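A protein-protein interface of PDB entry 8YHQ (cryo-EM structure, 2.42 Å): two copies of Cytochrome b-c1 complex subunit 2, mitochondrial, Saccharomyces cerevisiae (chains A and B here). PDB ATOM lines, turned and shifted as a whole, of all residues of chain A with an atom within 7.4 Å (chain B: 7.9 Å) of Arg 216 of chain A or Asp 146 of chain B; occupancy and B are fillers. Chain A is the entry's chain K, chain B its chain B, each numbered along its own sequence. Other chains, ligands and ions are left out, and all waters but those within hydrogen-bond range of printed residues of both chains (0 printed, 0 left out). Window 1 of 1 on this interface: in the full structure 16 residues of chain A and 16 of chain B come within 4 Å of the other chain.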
ATOM      1  N   ARG A 214     -24.913 -13.268   0.507  1.00  0.00           N
ATOM      2  CA  ARG A 214     -25.216 -14.237   1.608  1.00  0.00           C
ATOM      3  C   ARG A 214     -25.916 -13.517   2.788  1.00  0.00           C
ATOM      4  O   ARG A 214     -25.504 -12.455   3.123  1.00  0.00           O
ATOM      5  CB  ARG A 214     -23.999 -14.977   2.154  1.00  0.00           C
ATOM      6  CG  ARG A 214     -22.944 -15.317   1.120  1.00  0.00           C
ATOM      7  CD  ARG A 214     -21.677 -15.894   1.698  1.00  0.00           C
ATOM      8  NE  ARG A 214     -21.877 -17.224   2.219  1.00  0.00           N
ATOM      9  CZ  ARG A 214     -21.837 -18.330   1.505  1.00  0.00           C
ATOM     10  NH1 ARG A 214     -21.750 -19.485   2.113  1.00  0.00           N
ATOM     11  NH2 ARG A 214     -21.850 -18.282   0.190  1.00  0.00           N
ATOM     12  N   VAL A 215     -26.965 -14.049   3.372  1.00  0.00           N
ATOM     13  CA  VAL A 215     -27.797 -13.494   4.438  1.00  0.00           C
ATOM     14  C   VAL A 215     -27.981 -14.548   5.522  1.00  0.00           C
ATOM     15  O   VAL A 215     -28.343 -15.691   5.229  1.00  0.00           O
ATOM     16  CB  VAL A 215     -29.169 -13.025   3.913  1.00  0.00           C
ATOM     17  CG1 VAL A 215     -30.068 -12.627   5.054  1.00  0.00           C
ATOM     18  CG2 VAL A 215     -29.017 -11.873   2.945  1.00  0.00           C
ATOM     19  N   ARG A 216     -27.745 -14.159   6.773  1.00  0.00           N
ATOM     20  CA  ARG A 216     -27.960 -15.039   7.915  1.00  0.00           C
ATOM     21  C   ARG A 216     -29.424 -15.015   8.341  1.00  0.00           C
ATOM     22  O   ARG A 216     -30.080 -13.972   8.303  1.00  0.00           O
ATOM     23  CB  ARG A 216     -27.063 -14.624   9.080  1.00  0.00           C
ATOM     24  CG  ARG A 216     -25.583 -14.907   8.862  1.00  0.00           C
ATOM     25  CD  ARG A 216     -24.715 -14.378   9.988  1.00  0.00           C
ATOM     26  NE  ARG A 216     -24.605 -15.328  11.087  1.00  0.00           N
ATOM     27  CZ  ARG A 216     -23.772 -16.363  11.123  1.00  0.00           C
ATOM     28  NH1 ARG A 216     -23.777 -17.148  12.178  1.00  0.00           N
ATOM     29  NH2 ARG A 216     -22.932 -16.620  10.132  1.00  0.00           N
ATOM     30  N   PHE A 217     -29.932 -16.174   8.755  1.00  0.00           N
ATOM     31  CA  PHE A 217     -31.356 -16.343   9.000  1.00  0.00           C
ATOM     32  C   PHE A 217     -31.582 -17.596   9.834  1.00  0.00           C
ATOM     33  O   PHE A 217     -30.935 -18.620   9.610  1.00  0.00           O
ATOM     34  CB  PHE A 217     -32.110 -16.418   7.668  1.00  0.00           C
ATOM     35  CG  PHE A 217     -33.577 -16.678   7.798  1.00  0.00           C
ATOM     36  CD1 PHE A 217     -34.450 -15.646   8.052  1.00  0.00           C
ATOM     37  CD2 PHE A 217     -34.086 -17.950   7.634  1.00  0.00           C
ATOM     38  CE1 PHE A 217     -35.796 -15.880   8.162  1.00  0.00           C
ATOM     39  CE2 PHE A 217     -35.427 -18.181   7.744  1.00  0.00           C
ATOM     40  CZ  PHE A 217     -36.282 -17.145   8.006  1.00  0.00           C
ATOM     41  N   ILE A 218     -32.499 -17.502  10.796  1.00  0.00           N
ATOM     42  CA  ILE A 218     -32.875 -18.623  11.654  1.00  0.00           C
ATOM     43  C   ILE A 218     -34.039 -19.346  10.991  1.00  0.00           C
ATOM     44  O   ILE A 218     -35.097 -18.749  10.757  1.00  0.00           O
ATOM     45  CB  ILE A 218     -33.248 -18.159  13.075  1.00  0.00           C
ATOM     46  CG1 ILE A 218     -32.092 -17.376  13.708  1.00  0.00           C
ATOM     47  CG2 ILE A 218     -33.615 -19.363  13.966  1.00  0.00           C
ATOM     48  CD1 ILE A 218     -32.379 -16.773  15.040  1.00  0.00           C
ATOM     49  N   ALA A 339     -27.491 -17.032  -1.134  1.00  0.00           N
ATOM     50  CA  ALA A 339     -27.618 -18.028  -0.078  1.00  0.00           C
ATOM     51  C   ALA A 339     -28.272 -17.386   1.133  1.00  0.00           C
ATOM     52  O   ALA A 339     -27.937 -16.254   1.494  1.00  0.00           O
ATOM     53  CB  ALA A 339     -26.259 -18.613   0.295  1.00  0.00           C
ATOM     54  N   VAL A 340     -29.207 -18.106   1.749  1.00  0.00           N
ATOM     55  CA  VAL A 340     -29.949 -17.640   2.914  1.00  0.00           C
ATOM     56  C   VAL A 340     -29.950 -18.752   3.951  1.00  0.00           C
ATOM     57  O   VAL A 340     -30.206 -19.913   3.616  1.00  0.00           O
ATOM     58  CB  VAL A 340     -31.392 -17.234   2.560  1.00  0.00           C
ATOM     59  CG1 VAL A 340     -32.171 -16.903   3.803  1.00  0.00           C
ATOM     60  CG2 VAL A 340     -31.410 -16.059   1.614  1.00  0.00           C
ATOM     61  N   GLY A 341     -29.660 -18.396   5.200  1.00  0.00           N
ATOM     62  CA  GLY A 341     -29.705 -19.323   6.312  1.00  0.00           C
ATOM     63  C   GLY A 341     -28.384 -19.511   7.025  1.00  0.00           C
ATOM     64  O   GLY A 341     -27.741 -18.540   7.427  1.00  0.00           O
ATOM     65  N   ASP A 342     -27.982 -20.769   7.201  1.00  0.00           N
ATOM     66  CA  ASP A 342     -26.708 -21.115   7.830  1.00  0.00           C
ATOM     67  C   ASP A 342     -25.607 -20.977   6.785  1.00  0.00           C
ATOM     68  O   ASP A 342     -25.068 -21.951   6.258  1.00  0.00           O
ATOM     69  CB  ASP A 342     -26.762 -22.520   8.414  1.00  0.00           C
ATOM     70  CG  ASP A 342     -25.521 -22.878   9.199  1.00  0.00           C
ATOM     71  OD1 ASP A 342     -24.699 -21.977   9.472  1.00  0.00           O
ATOM     72  OD2 ASP A 342     -25.367 -24.065   9.548  1.00  0.00           O
ATOM     73  N   VAL A 343     -25.262 -19.722   6.494  1.00  0.00           N
ATOM     74  CA  VAL A 343     -24.343 -19.416   5.401  1.00  0.00           C
ATOM     75  C   VAL A 343     -22.906 -19.822   5.685  1.00  0.00           C
ATOM     76  O   VAL A 343     -22.087 -19.838   4.759  1.00  0.00           O
ATOM     77  CB  VAL A 343     -24.419 -17.919   5.040  1.00  0.00           C
ATOM     78  CG1 VAL A 343     -25.787 -17.592   4.499  1.00  0.00           C
ATOM     79  CG2 VAL A 343     -24.102 -17.021   6.224  1.00  0.00           C
ATOM     80  N   SER A 344     -22.571 -20.165   6.928  1.00  0.00           N
ATOM     81  CA  SER A 344     -21.251 -20.703   7.222  1.00  0.00           C
ATOM     82  C   SER A 344     -21.048 -22.104   6.669  1.00  0.00           C
ATOM     83  O   SER A 344     -19.901 -22.564   6.618  1.00  0.00           O
ATOM     84  CB  SER A 344     -21.014 -20.723   8.731  1.00  0.00           C
ATOM     85  OG  SER A 344     -20.931 -19.413   9.256  1.00  0.00           O
ATOM     86  N   ASN A 345     -22.120 -22.785   6.258  1.00  0.00           N
ATOM     87  CA  ASN A 345     -22.053 -24.150   5.759  1.00  0.00           C
ATOM     88  C   ASN A 345     -22.650 -24.301   4.362  1.00  0.00           C
ATOM     89  O   ASN A 345     -22.899 -25.433   3.934  1.00  0.00           O
ATOM     90  CB  ASN A 345     -22.763 -25.087   6.740  1.00  0.00           C
ATOM     91  CG  ASN A 345     -21.945 -25.356   7.981  1.00  0.00           C
ATOM     92  OD1 ASN A 345     -20.752 -25.641   7.905  1.00  0.00           O
ATOM     93  ND2 ASN A 345     -22.585 -25.266   9.137  1.00  0.00           N
ATOM     94  N   LYS B  28     -18.264 -24.126  16.185  1.00  0.00           N
ATOM     95  CA  LYS B  28     -19.578 -23.670  15.770  1.00  0.00           C
ATOM     96  C   LYS B  28     -19.693 -22.179  16.036  1.00  0.00           C
ATOM     97  O   LYS B  28     -18.920 -21.595  16.796  1.00  0.00           O
ATOM     98  CB  LYS B  28     -20.691 -24.432  16.497  1.00  0.00           C
ATOM     99  CG  LYS B  28     -20.750 -25.906  16.168  1.00  0.00           C
ATOM    100  CD  LYS B  28     -21.863 -26.610  16.909  1.00  0.00           C
ATOM    101  CE  LYS B  28     -21.887 -28.088  16.615  1.00  0.00           C
ATOM    102  NZ  LYS B  28     -22.158 -28.372  15.192  1.00  0.00           N
ATOM    103  N   ASP B  29     -20.680 -21.568  15.398  1.00  0.00           N
ATOM    104  CA  ASP B  29     -20.875 -20.127  15.477  1.00  0.00           C
ATOM    105  C   ASP B  29     -21.329 -19.758  16.882  1.00  0.00           C
ATOM    106  O   ASP B  29     -22.488 -19.954  17.249  1.00  0.00           O
ATOM    107  CB  ASP B  29     -21.885 -19.671  14.433  1.00  0.00           C
ATOM    108  CG  ASP B  29     -21.376 -19.827  13.020  1.00  0.00           C
ATOM    109  OD1 ASP B  29     -20.230 -20.286  12.843  1.00  0.00           O
ATOM    110  OD2 ASP B  29     -22.122 -19.486  12.081  1.00  0.00           O
ATOM    111  N   GLY B  30     -20.402 -19.231  17.673  1.00  0.00           N
ATOM    112  CA  GLY B  30     -20.701 -18.656  18.964  1.00  0.00           C
ATOM    113  C   GLY B  30     -20.296 -19.467  20.171  1.00  0.00           C
ATOM    114  O   GLY B  30     -20.688 -19.110  21.285  1.00  0.00           O
ATOM    115  N   HIS B  33     -17.928 -17.373  22.489  1.00  0.00           N
ATOM    116  CA  HIS B  33     -18.647 -16.348  23.238  1.00  0.00           C
ATOM    117  C   HIS B  33     -19.335 -16.937  24.459  1.00  0.00           C
ATOM    118  O   HIS B  33     -19.349 -16.321  25.529  1.00  0.00           O
ATOM    119  CB  HIS B  33     -19.658 -15.658  22.324  1.00  0.00           C
ATOM    120  CG  HIS B  33     -20.468 -14.592  22.992  1.00  0.00           C
ATOM    121  ND1 HIS B  33     -21.692 -14.190  22.509  1.00  0.00           N
ATOM    122  CD2 HIS B  33     -20.229 -13.833  24.085  1.00  0.00           C
ATOM    123  CE1 HIS B  33     -22.176 -13.237  23.281  1.00  0.00           C
ATOM    124  NE2 HIS B  33     -21.311 -13.004  24.247  1.00  0.00           N
ATOM    125  N   LEU B  34     -19.922 -18.122  24.323  1.00  0.00           N
ATOM    126  CA  LEU B  34     -20.609 -18.725  25.456  1.00  0.00           C
ATOM    127  C   LEU B  34     -19.623 -19.178  26.524  1.00  0.00           C
ATOM    128  O   LEU B  34     -19.820 -18.883  27.705  1.00  0.00           O
ATOM    129  CB  LEU B  34     -21.490 -19.880  24.982  1.00  0.00           C
ATOM    130  CG  LEU B  34     -22.650 -19.513  24.047  1.00  0.00           C
ATOM    131  CD1 LEU B  34     -23.420 -20.730  23.657  1.00  0.00           C
ATOM    132  CD2 LEU B  34     -23.584 -18.509  24.656  1.00  0.00           C
ATOM    133  N   ALA B 111     -25.523 -13.541  27.113  1.00  0.00           N
ATOM    134  CA  ALA B 111     -25.154 -13.543  25.705  1.00  0.00           C
ATOM    135  C   ALA B 111     -26.225 -12.883  24.848  1.00  0.00           C
ATOM    136  O   ALA B 111     -25.910 -12.212  23.859  1.00  0.00           O
ATOM    137  CB  ALA B 111     -24.890 -14.972  25.240  1.00  0.00           C
ATOM    138  N   ARG B 112     -27.498 -13.069  25.202  1.00  0.00           N
ATOM    139  CA  ARG B 112     -28.573 -12.381  24.498  1.00  0.00           C
ATOM    140  C   ARG B 112     -28.443 -10.870  24.633  1.00  0.00           C
ATOM    141  O   ARG B 112     -28.753 -10.127  23.697  1.00  0.00           O
ATOM    142  CB  ARG B 112     -29.931 -12.836  25.025  1.00  0.00           C
ATOM    143  CG  ARG B 112     -30.430 -14.159  24.478  1.00  0.00           C
ATOM    144  CD  ARG B 112     -31.915 -14.381  24.753  1.00  0.00           C
ATOM    145  NE  ARG B 112     -32.185 -14.987  26.057  1.00  0.00           N
ATOM    146  CZ  ARG B 112     -32.271 -16.294  26.302  1.00  0.00           C
ATOM    147  NH1 ARG B 112     -32.533 -16.700  27.533  1.00  0.00           N
ATOM    148  NH2 ARG B 112     -32.094 -17.201  25.346  1.00  0.00           N
ATOM    149  N   TYR B 115     -25.486  -9.503  22.351  1.00  0.00           N
ATOM    150  CA  TYR B 115     -25.857  -9.448  20.941  1.00  0.00           C
ATOM    151  C   TYR B 115     -26.815  -8.298  20.660  1.00  0.00           C
ATOM    152  O   TYR B 115     -26.625  -7.540  19.703  1.00  0.00           O
ATOM    153  CB  TYR B 115     -26.468 -10.779  20.512  1.00  0.00           C
ATOM    154  CG  TYR B 115     -26.931 -10.802  19.081  1.00  0.00           C
ATOM    155  CD1 TYR B 115     -26.026 -10.922  18.044  1.00  0.00           C
ATOM    156  CD2 TYR B 115     -28.271 -10.696  18.765  1.00  0.00           C
ATOM    157  CE1 TYR B 115     -26.443 -10.936  16.743  1.00  0.00           C
ATOM    158  CE2 TYR B 115     -28.696 -10.709  17.468  1.00  0.00           C
ATOM    159  CZ  TYR B 115     -27.778 -10.830  16.457  1.00  0.00           C
ATOM    160  OH  TYR B 115     -28.198 -10.847  15.152  1.00  0.00           O
ATOM    161  N   ASP B 128     -18.049  -6.664  10.860  1.00  0.00           N
ATOM    162  CA  ASP B 128     -18.220  -8.105  10.691  1.00  0.00           C
ATOM    163  C   ASP B 128     -18.351  -8.490   9.225  1.00  0.00           C
ATOM    164  O   ASP B 128     -17.862  -9.545   8.808  1.00  0.00           O
ATOM    165  CB  ASP B 128     -19.442  -8.591  11.468  1.00  0.00           C
ATOM    166  CG  ASP B 128     -19.224  -9.939  12.148  1.00  0.00           C
ATOM    167  OD1 ASP B 128     -18.241 -10.647  11.835  1.00  0.00           O
ATOM    168  OD2 ASP B 128     -20.054 -10.304  13.011  1.00  0.00           O
ATOM    169  N   GLN B 129     -19.027  -7.661   8.428  1.00  0.00           N
ATOM    170  CA  GLN B 129     -19.196  -7.971   7.015  1.00  0.00           C
ATOM    171  C   GLN B 129     -17.866  -7.940   6.273  1.00  0.00           C
ATOM    172  O   GLN B 129     -17.591  -8.821   5.453  1.00  0.00           O
ATOM    173  CB  GLN B 129     -20.194  -6.999   6.388  1.00  0.00           C
ATOM    174  CG  GLN B 129     -21.637  -7.168   6.849  1.00  0.00           C
ATOM    175  CD  GLN B 129     -22.232  -8.501   6.476  1.00  0.00           C
ATOM    176  OE1 GLN B 129     -22.723  -9.233   7.330  1.00  0.00           O
ATOM    177  NE2 GLN B 129     -22.197  -8.825   5.195  1.00  0.00           N
ATOM    178  N   ALA B 132     -16.112 -10.947   6.886  1.00  0.00           N
ATOM    179  CA  ALA B 132     -16.755 -12.135   6.340  1.00  0.00           C
ATOM    180  C   ALA B 132     -16.509 -12.286   4.844  1.00  0.00           C
ATOM    181  O   ALA B 132     -16.452 -13.414   4.345  1.00  0.00           O
ATOM    182  CB  ALA B 132     -18.252 -12.091   6.623  1.00  0.00           C
ATOM    183  N   GLY B 140     -12.898 -14.588   9.602  1.00  0.00           N
ATOM    184  CA  GLY B 140     -14.229 -14.171   9.227  1.00  0.00           C
ATOM    185  C   GLY B 140     -15.372 -14.848   9.942  1.00  0.00           C
ATOM    186  O   GLY B 140     -16.528 -14.550   9.636  1.00  0.00           O
ATOM    187  N   ASN B 141     -15.098 -15.753  10.875  1.00  0.00           N
ATOM    188  CA  ASN B 141     -16.167 -16.358  11.649  1.00  0.00           C
ATOM    189  C   ASN B 141     -16.877 -15.294  12.486  1.00  0.00           C
ATOM    190  O   ASN B 141     -16.288 -14.260  12.812  1.00  0.00           O
ATOM    191  CB  ASN B 141     -15.628 -17.445  12.567  1.00  0.00           C
ATOM    192  CG  ASN B 141     -15.117 -18.644  11.820  1.00  0.00           C
ATOM    193  OD1 ASN B 141     -15.428 -18.850  10.649  1.00  0.00           O
ATOM    194  ND2 ASN B 141     -14.331 -19.454  12.500  1.00  0.00           N
ATOM    195  N   PRO B 142     -18.141 -15.516  12.855  1.00  0.00           N
ATOM    196  CA  PRO B 142     -18.825 -14.535  13.702  1.00  0.00           C
ATOM    197  C   PRO B 142     -18.229 -14.484  15.097  1.00  0.00           C
ATOM    198  O   PRO B 142     -17.671 -15.460  15.601  1.00  0.00           O
ATOM    199  CB  PRO B 142     -20.274 -15.032  13.740  1.00  0.00           C
ATOM    200  CG  PRO B 142     -20.378 -16.071  12.764  1.00  0.00           C
ATOM    201  CD  PRO B 142     -19.039 -16.624  12.496  1.00  0.00           C
ATOM    202  N   LEU B 143     -18.365 -13.319  15.723  1.00  0.00           N
ATOM    203  CA  LEU B 143     -17.875 -13.087  17.072  1.00  0.00           C
ATOM    204  C   LEU B 143     -18.882 -13.529  18.129  1.00  0.00           C
ATOM    205  O   LEU B 143     -18.537 -14.296  19.032  1.00  0.00           O
ATOM    206  CB  LEU B 143     -17.538 -11.605  17.235  1.00  0.00           C
ATOM    207  CG  LEU B 143     -16.735 -11.157  18.453  1.00  0.00           C
ATOM    208  CD1 LEU B 143     -15.319 -11.679  18.419  1.00  0.00           C
ATOM    209  CD2 LEU B 143     -16.733  -9.655  18.524  1.00  0.00           C
ATOM    210  N   LEU B 144     -20.125 -13.070  18.016  1.00  0.00           N
ATOM    211  CA  LEU B 144     -21.154 -13.301  19.019  1.00  0.00           C
ATOM    212  C   LEU B 144     -22.171 -14.339  18.561  1.00  0.00           C
ATOM    213  O   LEU B 144     -22.386 -14.559  17.367  1.00  0.00           O
ATOM    214  CB  LEU B 144     -21.871 -11.994  19.361  1.00  0.00           C
ATOM    215  CG  LEU B 144     -21.014 -10.804  19.795  1.00  0.00           C
ATOM    216  CD1 LEU B 144     -21.896  -9.675  20.234  1.00  0.00           C
ATOM    217  CD2 LEU B 144     -20.028 -11.151  20.899  1.00  0.00           C
ATOM    218  N   TYR B 145     -22.797 -14.975  19.548  1.00  0.00           N
ATOM    219  CA  TYR B 145     -23.815 -15.993  19.337  1.00  0.00           C
ATOM    220  C   TYR B 145     -25.170 -15.345  19.082  1.00  0.00           C
ATOM    221  O   TYR B 145     -25.613 -14.493  19.857  1.00  0.00           O
ATOM    222  CB  TYR B 145     -23.867 -16.899  20.563  1.00  0.00           C
ATOM    223  CG  TYR B 145     -24.943 -17.957  20.589  1.00  0.00           C
ATOM    224  CD1 TYR B 145     -24.712 -19.218  20.071  1.00  0.00           C
ATOM    225  CD2 TYR B 145     -26.172 -17.711  21.175  1.00  0.00           C
ATOM    226  CE1 TYR B 145     -25.679 -20.188  20.109  1.00  0.00           C
ATOM    227  CE2 TYR B 145     -27.142 -18.674  21.215  1.00  0.00           C
ATOM    228  CZ  TYR B 145     -26.892 -19.911  20.684  1.00  0.00           C
ATOM    229  OH  TYR B 145     -27.864 -20.879  20.726  1.00  0.00           O
ATOM    230  N   ASP B 146     -25.825 -15.760  17.992  1.00  0.00           N
ATOM    231  CA  ASP B 146     -27.131 -15.249  17.599  1.00  0.00           C
ATOM    232  C   ASP B 146     -28.204 -16.319  17.475  1.00  0.00           C
ATOM    233  O   ASP B 146     -29.384 -15.967  17.380  1.00  0.00           O
ATOM    234  CB  ASP B 146     -27.031 -14.496  16.265  1.00  0.00           C
ATOM    235  CG  ASP B 146     -26.452 -15.340  15.154  1.00  0.00           C
ATOM    236  OD1 ASP B 146     -25.867 -16.402  15.442  1.00  0.00           O
ATOM    237  OD2 ASP B 146     -26.572 -14.930  13.984  1.00  0.00           O
ATOM    238  N   GLY B 147     -27.841 -17.598  17.456  1.00  0.00           N
ATOM    239  CA  GLY B 147     -28.796 -18.680  17.479  1.00  0.00           C
ATOM    240  C   GLY B 147     -29.117 -19.328  16.149  1.00  0.00           C
ATOM    241  O   GLY B 147     -29.942 -20.247  16.120  1.00  0.00           O
ATOM    242  N   VAL B 148     -28.500 -18.894  15.047  1.00  0.00           N
ATOM    243  CA  VAL B 148     -28.748 -19.538  13.762  1.00  0.00           C
ATOM    244  C   VAL B 148     -28.166 -20.940  13.706  1.00  0.00           C
ATOM    245  O   VAL B 148     -28.573 -21.736  12.855  1.00  0.00           O
ATOM    246  CB  VAL B 148     -28.196 -18.702  12.583  1.00  0.00           C
ATOM    247  CG1 VAL B 148     -28.733 -17.277  12.620  1.00  0.00           C
ATOM    248  CG2 VAL B 148     -26.701 -18.701  12.561  1.00  0.00           C
ATOM    249  N   GLU B 149     -27.217 -21.251  14.584  1.00  0.00           N
ATOM    250  CA  GLU B 149     -26.655 -22.584  14.729  1.00  0.00           C
ATOM    251  C   GLU B 149     -26.744 -22.975  16.196  1.00  0.00           C
ATOM    252  O   GLU B 149     -26.291 -22.228  17.068  1.00  0.00           O
ATOM    253  CB  GLU B 149     -25.208 -22.618  14.227  1.00  0.00           C
ATOM    254  CG  GLU B 149     -24.695 -23.989  13.841  1.00  0.00           C
ATOM    255  CD  GLU B 149     -23.370 -23.943  13.097  1.00  0.00           C
ATOM    256  OE1 GLU B 149     -22.965 -22.854  12.644  1.00  0.00           O
ATOM    257  OE2 GLU B 149     -22.728 -25.005  12.964  1.00  0.00           O
ATOM    258  N   VAL B 151     -26.112 -24.481  19.694  1.00  0.00           N
ATOM    259  CA  VAL B 151     -24.943 -24.830  20.497  1.00  0.00           C
ATOM    260  C   VAL B 151     -25.434 -25.425  21.807  1.00  0.00           C
ATOM    261  O   VAL B 151     -26.136 -24.759  22.576  1.00  0.00           O
ATOM    262  CB  VAL B 151     -24.035 -23.614  20.745  1.00  0.00           C
ATOM    263  CG1 VAL B 151     -22.832 -23.994  21.602  1.00  0.00           C
ATOM    264  CG2 VAL B 151     -23.562 -23.024  19.438  1.00  0.00           C
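The guanidinium group of Arg 216 of chain A is in salt-bridge range of the side-chain carboxylate of Asp 29 of chain B. OD2 of Asp 29 of chain B lies within hydrogen-bond range of OG of Ser 344 of chain A (3.1 Å). OD2 of Asp 146 of chain B is in salt-bridge range of NE of Arg 216 of chain A (3.5 Å).
N of Phe 217 of chain A lies within hydrogen-bond range of O of Gly 341 of chain A (3.5 Å). OD2 of Asp 342 of chain A lies within hydrogen-bond range of ND2 of Asn 345 of chain A, at 3.1 Å.
Among the printed residues, merely in contact across the chains: Arg 216 of chain A with Val 148 of chain B (3.3 Å), Ile 218 of chain A with Val 148 of chain B (3.5 Å), Arg 216 of chain A with Pro 142 of chain B (3.6 Å), Asp 342 of chain A with Glu 149 of chain B (3.7 Å), Asn 345 of chain A with Glu 149 of chain B (3.8 Å), Ile 218 of chain A with Asp 146 of chain B (3.9 Å) and Phe 217 of chain A with Val 148 of chain B (3.96 Å).
Arg 216 of chain A touches just these residues of chain B: Asp 29, Pro 142, Asp 146 and Val 148. Of the printed residues of chain B, Phe 217 of chain A touches Val 148 (3.96 Å). Of the printed residues of chain B, Ser 344 of chain A touches Asp 29 (3.1 Å). Of the printed residues of chain A, Asp 29 of chain B touches Arg 216 and Ser 344. Asp 146 of chain B touches just these residues of chain A: Arg 216 and Ile 218. Val 151 of chain B touches none of the printed residues of chain A. The nearest residue of chain A that does not touch Asp 146 of chain B is Phe 217 of chain A (6.3 Å). The nearest printed residue of chain A that does not touch Glu 149 of chain B is Ser 344 of chain A (4.9 Å).
Printed residues of chain B that touch a printed residue of chain A: Asp 29, Pro 142, Asp 146, Val 148 and Glu 149. Among the printed residues, 10 pairs touch across the chains. Among the printed residues, Asp or Glu carboxylates within 4 Å of a Lys or Arg side-chain nitrogen of the other chain: Arg 216 of chain A with Asp 29 of chain B (2.9 Å) and Arg 216 of chain A with Asp 146 of chain B (3.5 Å).
No position is printed for both chains.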
